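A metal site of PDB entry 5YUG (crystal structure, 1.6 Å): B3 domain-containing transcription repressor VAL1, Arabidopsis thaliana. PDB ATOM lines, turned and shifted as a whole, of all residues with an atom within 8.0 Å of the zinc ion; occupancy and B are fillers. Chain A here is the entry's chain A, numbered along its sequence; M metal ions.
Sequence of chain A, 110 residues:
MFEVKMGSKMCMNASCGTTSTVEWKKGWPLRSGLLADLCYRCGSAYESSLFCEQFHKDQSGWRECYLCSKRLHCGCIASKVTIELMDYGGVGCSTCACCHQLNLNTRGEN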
ATOM      1  N   MET A  10       5.999  23.628  -8.316  1.00  0.00           N
ATOM      2  CA  MET A  10       6.332  22.860  -7.123  1.00  0.00           C
ATOM      3  C   MET A  10       7.401  23.627  -6.359  1.00  0.00           C
ATOM      4  O   MET A  10       8.359  24.123  -6.943  1.00  0.00           O
ATOM      5  CB  MET A  10       6.810  21.459  -7.479  1.00  0.00           C
ATOM      6  CG  MET A  10       7.146  20.633  -6.268  1.00  0.00           C
ATOM      7  SD  MET A  10       7.301  18.913  -6.742  1.00  0.00           S
ATOM      8  CE  MET A  10       8.261  18.298  -5.386  1.00  0.00           C
ATOM      9  N   CYS A  11       7.216  23.734  -5.038  1.00  0.00           N
ATOM     10  CA  CYS A  11       8.189  24.450  -4.215  1.00  0.00           C
ATOM     11  C   CYS A  11       9.570  23.836  -4.381  1.00  0.00           C
ATOM     12  O   CYS A  11       9.743  22.619  -4.220  1.00  0.00           O
ATOM     13  CB  CYS A  11       7.768  24.413  -2.757  1.00  0.00           C
ATOM     14  SG  CYS A  11       8.821  25.521  -1.753  1.00  0.00           S
ATOM     15  N   MET A  12      10.562  24.672  -4.712  1.00  0.00           N
ATOM     16  CA  MET A  12      11.920  24.195  -4.926  1.00  0.00           C
ATOM     17  C   MET A  12      12.742  24.164  -3.638  1.00  0.00           C
ATOM     18  O   MET A  12      13.935  23.838  -3.681  1.00  0.00           O
ATOM     19  CB  MET A  12      12.632  25.053  -5.981  1.00  0.00           C
ATOM     20  CG  MET A  12      12.013  24.852  -7.350  1.00  0.00           C
ATOM     21  SD  MET A  12      12.727  25.895  -8.629  1.00  0.00           S
ATOM     22  CE  MET A  12      11.606  25.517  -9.977  1.00  0.00           C
ATOM     23  N   ASN A  13      12.133  24.462  -2.495  1.00  0.00           N
ATOM     24  CA  ASN A  13      12.748  24.122  -1.216  1.00  0.00           C
ATOM     25  C   ASN A  13      12.576  22.618  -1.028  1.00  0.00           C
ATOM     26  O   ASN A  13      11.460  22.126  -0.892  1.00  0.00           O
ATOM     27  CB  ASN A  13      12.123  24.903  -0.078  1.00  0.00           C
ATOM     28  CG  ASN A  13      12.558  24.403   1.290  1.00  0.00           C
ATOM     29  OD1 ASN A  13      13.575  23.716   1.412  1.00  0.00           O
ATOM     30  ND2 ASN A  13      11.822  24.795   2.326  1.00  0.00           N
ATOM     31  N   ALA A  14      13.703  21.891  -1.045  1.00  0.00           N
ATOM     32  CA  ALA A  14      13.679  20.450  -1.205  1.00  0.00           C
ATOM     33  C   ALA A  14      13.039  19.739  -0.014  1.00  0.00           C
ATOM     34  O   ALA A  14      12.542  18.621  -0.181  1.00  0.00           O
ATOM     35  CB  ALA A  14      15.104  19.941  -1.416  1.00  0.00           C
ATOM     36  N   SER A  15      13.022  20.354   1.163  1.00  0.00           N
ATOM     37  CA  SER A  15      12.312  19.746   2.279  1.00  0.00           C
ATOM     38  C   SER A  15      10.814  20.035   2.264  1.00  0.00           C
ATOM     39  O   SER A  15      10.088  19.505   3.101  1.00  0.00           O
ATOM     40  CB  SER A  15      12.895  20.228   3.606  1.00  0.00           C
ATOM     41  OG  SER A  15      12.720  21.622   3.740  1.00  0.00           O
ATOM     42  N   CYS A  16      10.344  20.861   1.323  1.00  0.00           N
ATOM     43  CA  CYS A  16       8.936  21.201   1.198  1.00  0.00           C
ATOM     44  C   CYS A  16       8.310  20.466   0.018  1.00  0.00           C
ATOM     45  O   CYS A  16       7.472  19.564   0.204  1.00  0.00           O
ATOM     46  CB  CYS A  16       8.787  22.713   1.058  1.00  0.00           C
ATOM     47  SG  CYS A  16       7.104  23.304   0.789  1.00  0.00           S
ATOM     48  N   GLY A  17       8.689  20.831  -1.198  1.00  0.00           N
ATOM     49  CA  GLY A  17       8.156  20.218  -2.397  1.00  0.00           C
ATOM     50  C   GLY A  17       6.651  20.316  -2.566  1.00  0.00           C
ATOM     51  O   GLY A  17       6.073  19.515  -3.308  1.00  0.00           O
ATOM     52  N   THR A  18       5.985  21.276  -1.931  1.00  0.00           N
ATOM     53  CA  THR A  18       4.537  21.346  -2.057  1.00  0.00           C
ATOM     54  C   THR A  18       4.114  21.838  -3.444  1.00  0.00           C
ATOM     55  O   THR A  18       4.820  22.595  -4.114  1.00  0.00           O
ATOM     56  CB  THR A  18       3.928  22.226  -0.970  1.00  0.00           C
ATOM     57  OG1 THR A  18       2.511  21.971  -0.900  1.00  0.00           O
ATOM     58  CG2 THR A  18       4.135  23.708  -1.273  1.00  0.00           C
ATOM     59  N   THR A  19       2.935  21.389  -3.875  1.00  0.00           N
ATOM     60  CA  THR A  19       2.315  21.841  -5.109  1.00  0.00           C
ATOM     61  C   THR A  19       1.057  22.638  -4.842  1.00  0.00           C
ATOM     62  O   THR A  19       0.397  23.087  -5.793  1.00  0.00           O
ATOM     63  CB  THR A  19       1.961  20.642  -5.992  1.00  0.00           C
ATOM     64  OG1 THR A  19       1.077  19.778  -5.268  1.00  0.00           O
ATOM     65  CG2 THR A  19       3.220  19.886  -6.390  1.00  0.00           C
ATOM     66  N   SER A  20       0.713  22.839  -3.580  1.00  0.00           N
ATOM     67  CA  SER A  20      -0.541  23.465  -3.166  1.00  0.00           C
ATOM     68  C   SER A  20      -0.202  24.607  -2.213  1.00  0.00           C
ATOM     69  O   SER A  20       0.344  24.370  -1.121  1.00  0.00           O
ATOM     70  CB  SER A  20      -1.458  22.422  -2.514  1.00  0.00           C
ATOM     71  OG  SER A  20      -2.297  22.957  -1.500  1.00  0.00           O
ATOM     72  N   THR A  21      -0.487  25.845  -2.622  1.00  0.00           N
ATOM     73  CA  THR A  21      -0.166  27.012  -1.800  1.00  0.00           C
ATOM     74  C   THR A  21      -1.125  28.145  -2.150  1.00  0.00           C
ATOM     75  O   THR A  21      -1.650  28.210  -3.258  1.00  0.00           O
ATOM     76  CB  THR A  21       1.288  27.453  -2.017  1.00  0.00           C
ATOM     77  OG1 THR A  21       1.610  28.490  -1.080  1.00  0.00           O
ATOM     78  CG2 THR A  21       1.523  27.950  -3.449  1.00  0.00           C
ATOM     79  N   TRP A  24       2.086  31.648  -5.066  1.00  0.00           N
ATOM     80  CA  TRP A  24       3.435  31.316  -5.484  1.00  0.00           C
ATOM     81  C   TRP A  24       4.323  32.550  -5.460  1.00  0.00           C
ATOM     82  O   TRP A  24       3.914  33.651  -5.860  1.00  0.00           O
ATOM     83  CB  TRP A  24       3.424  30.677  -6.867  1.00  0.00           C
ATOM     84  CG  TRP A  24       2.892  29.290  -6.835  1.00  0.00           C
ATOM     85  CD1 TRP A  24       1.666  28.878  -7.252  1.00  0.00           C
ATOM     86  CD2 TRP A  24       3.560  28.130  -6.323  1.00  0.00           C
ATOM     87  NE1 TRP A  24       1.525  27.529  -7.034  1.00  0.00           N
ATOM     88  CE2 TRP A  24       2.684  27.042  -6.476  1.00  0.00           C
ATOM     89  CE3 TRP A  24       4.817  27.916  -5.760  1.00  0.00           C
ATOM     90  CZ2 TRP A  24       3.021  25.752  -6.080  1.00  0.00           C
ATOM     91  CZ3 TRP A  24       5.158  26.638  -5.368  1.00  0.00           C
ATOM     92  CH2 TRP A  24       4.256  25.573  -5.528  1.00  0.00           C
ATOM     93  N   ASP A  37      11.103  28.837  -7.889  1.00  0.00           N
ATOM     94  CA  ASP A  37       9.736  28.844  -7.401  1.00  0.00           C
ATOM     95  C   ASP A  37       9.700  28.423  -5.945  1.00  0.00           C
ATOM     96  O   ASP A  37      10.273  27.401  -5.571  1.00  0.00           O
ATOM     97  CB  ASP A  37       8.862  27.897  -8.232  1.00  0.00           C
ATOM     98  CG  ASP A  37       8.601  28.408  -9.638  1.00  0.00           C
ATOM     99  OD1 ASP A  37       8.415  29.627  -9.846  1.00  0.00           O
ATOM    100  OD2 ASP A  37       8.585  27.555 -10.545  1.00  0.00           O
ATOM    101  N   LEU A  38       9.003  29.204  -5.119  1.00  0.00           N
ATOM    102  CA  LEU A  38       8.823  28.898  -3.707  1.00  0.00           C
ATOM    103  C   LEU A  38       7.354  29.100  -3.350  1.00  0.00           C
ATOM    104  O   LEU A  38       6.715  30.035  -3.853  1.00  0.00           O
ATOM    105  CB  LEU A  38       9.708  29.782  -2.822  1.00  0.00           C
ATOM    106  CG  LEU A  38      11.228  29.604  -2.861  1.00  0.00           C
ATOM    107  CD1 LEU A  38      11.862  30.590  -1.869  1.00  0.00           C
ATOM    108  CD2 LEU A  38      11.680  28.163  -2.576  1.00  0.00           C
ATOM    109  N   CYS A  39       6.828  28.232  -2.485  1.00  0.00           N
ATOM    110  CA  CYS A  39       5.457  28.422  -2.011  1.00  0.00           C
ATOM    111  C   CYS A  39       5.378  29.656  -1.111  1.00  0.00           C
ATOM    112  O   CYS A  39       6.383  30.289  -0.771  1.00  0.00           O
ATOM    113  CB  CYS A  39       4.978  27.178  -1.274  1.00  0.00           C
ATOM    114  SG  CYS A  39       5.810  26.878   0.325  1.00  0.00           S
ATOM    115  N   TYR A  40       4.147  30.021  -0.728  1.00  0.00           N
ATOM    116  CA  TYR A  40       3.936  31.189   0.133  1.00  0.00           C
ATOM    117  C   TYR A  40       4.806  31.134   1.392  1.00  0.00           C
ATOM    118  O   TYR A  40       5.433  32.117   1.772  1.00  0.00           O
ATOM    119  CB  TYR A  40       2.473  31.304   0.525  1.00  0.00           C
ATOM    120  CG  TYR A  40       2.202  32.588   1.284  1.00  0.00           C
ATOM    121  CD1 TYR A  40       2.054  33.773   0.616  1.00  0.00           C
ATOM    122  CD2 TYR A  40       2.126  32.584   2.674  1.00  0.00           C
ATOM    123  CE1 TYR A  40       1.834  34.950   1.284  1.00  0.00           C
ATOM    124  CE2 TYR A  40       1.892  33.764   3.369  1.00  0.00           C
ATOM    125  CZ  TYR A  40       1.753  34.946   2.661  1.00  0.00           C
ATOM    126  OH  TYR A  40       1.528  36.134   3.300  1.00  0.00           O
ATOM    127  N   ARG A  41       4.816  29.975   2.052  1.00  0.00           N
ATOM    128  CA  ARG A  41       5.588  29.772   3.274  1.00  0.00           C
ATOM    129  C   ARG A  41       7.088  29.968   3.039  1.00  0.00           C
ATOM    130  O   ARG A  41       7.734  30.820   3.671  1.00  0.00           O
ATOM    131  CB  ARG A  41       5.272  28.371   3.811  1.00  0.00           C
ATOM    132  CG  ARG A  41       6.063  27.912   5.017  1.00  0.00           C
ATOM    133  CD  ARG A  41       5.446  26.613   5.573  1.00  0.00           C
ATOM    134  NE  ARG A  41       5.712  25.458   4.723  1.00  0.00           N
ATOM    135  CZ  ARG A  41       6.752  24.646   4.914  1.00  0.00           C
ATOM    136  NH1 ARG A  41       7.589  24.861   5.899  1.00  0.00           N
ATOM    137  NH2 ARG A  41       6.950  23.617   4.106  1.00  0.00           N
ATOM    138  N   CYS A  42       7.650  29.168   2.133  1.00  0.00           N
ATOM    139  CA  CYS A  42       9.101  29.216   1.912  1.00  0.00           C
ATOM    140  C   CYS A  42       9.529  30.519   1.255  1.00  0.00           C
ATOM    141  O   CYS A  42      10.590  31.070   1.560  1.00  0.00           O
ATOM    142  CB  CYS A  42       9.539  28.006   1.074  1.00  0.00           C
ATOM    143  SG  CYS A  42       9.045  26.440   1.820  1.00  0.00           S
ATOM    144  N   GLY A  43       8.710  31.019   0.340  1.00  0.00           N
ATOM    145  CA  GLY A  43       9.017  32.317  -0.260  1.00  0.00           C
ATOM    146  C   GLY A  43       8.957  33.437   0.755  1.00  0.00           C
ATOM    147  O   GLY A  43       9.738  34.391   0.681  1.00  0.00           O
ATOM    148  N   PHE A  51      15.505  32.339   5.289  1.00  0.00           N
ATOM    149  CA  PHE A  51      15.305  31.010   4.723  1.00  0.00           C
ATOM    150  C   PHE A  51      16.227  29.982   5.362  1.00  0.00           C
ATOM    151  O   PHE A  51      15.779  28.899   5.783  1.00  0.00           O
ATOM    152  CB  PHE A  51      15.494  31.057   3.194  1.00  0.00           C
ATOM    153  CG  PHE A  51      15.204  29.737   2.509  1.00  0.00           C
ATOM    154  CD1 PHE A  51      16.194  28.777   2.377  1.00  0.00           C
ATOM    155  CD2 PHE A  51      13.945  29.460   1.979  1.00  0.00           C
ATOM    156  CE1 PHE A  51      15.938  27.548   1.747  1.00  0.00           C
ATOM    157  CE2 PHE A  51      13.686  28.254   1.341  1.00  0.00           C
ATOM    158  CZ  PHE A  51      14.676  27.293   1.247  1.00  0.00           C
ATOM    159  N   PHE A  55      15.173  26.668   7.565  1.00  0.00           N
ATOM    160  CA  PHE A  55      15.205  25.352   6.927  1.00  0.00           C
ATOM    161  C   PHE A  55      16.547  24.628   6.941  1.00  0.00           C
ATOM    162  O   PHE A  55      16.567  23.417   6.703  1.00  0.00           O
ATOM    163  CB  PHE A  55      14.748  25.456   5.464  1.00  0.00           C
ATOM    164  CG  PHE A  55      13.345  25.963   5.301  1.00  0.00           C
ATOM    165  CD1 PHE A  55      12.276  25.216   5.771  1.00  0.00           C
ATOM    166  CD2 PHE A  55      13.077  27.174   4.687  1.00  0.00           C
ATOM    167  CE1 PHE A  55      10.983  25.654   5.622  1.00  0.00           C
ATOM    168  CE2 PHE A  55      11.770  27.610   4.535  1.00  0.00           C
ATOM    169  CZ  PHE A  55      10.737  26.859   5.016  1.00  0.00           C
HETATM  170 ZN    ZN M   1       7.639  25.444   0.208  1.00  0.00          ZN
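The backbone carbonyl oxygen of Thr 18 sits at hydrogen-bond distance from the backbone NH of Cys 11 (2.8 Å).
The side-chain sulfur of Cys 39 sits close to the backbone NH of Arg 41, 3.7 Å away.
N of Asn 13 sits close to SG of Cys 11, at 3.6 Å.
The side-chain sulfur (SG) of Cys 16 sits close to the backbone NH (N) of Thr 18 (3.6 Å).
The side-chain amide nitrogen (ND2) of Asn 13 lies close to the side-chain sulfur (SG) of Cys 42.
The side-chain sulfur of Cys 16 lies close to the guanidinium group of Arg 41, 3.3 Å away.
SG of Cys 16 is bound to the zinc ion, 2.3 Å away.
The zinc ion is bound by SG of Cys 11.
SG of Cys 39 binds the zinc ion, at 2.3 Å.
SG of Cys 42 is bound to the zinc ion.
The zinc ion has four donor atoms within binding distance.
Along chain A the residues within 4 Å of the zinc ion span positions 11 to 42.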
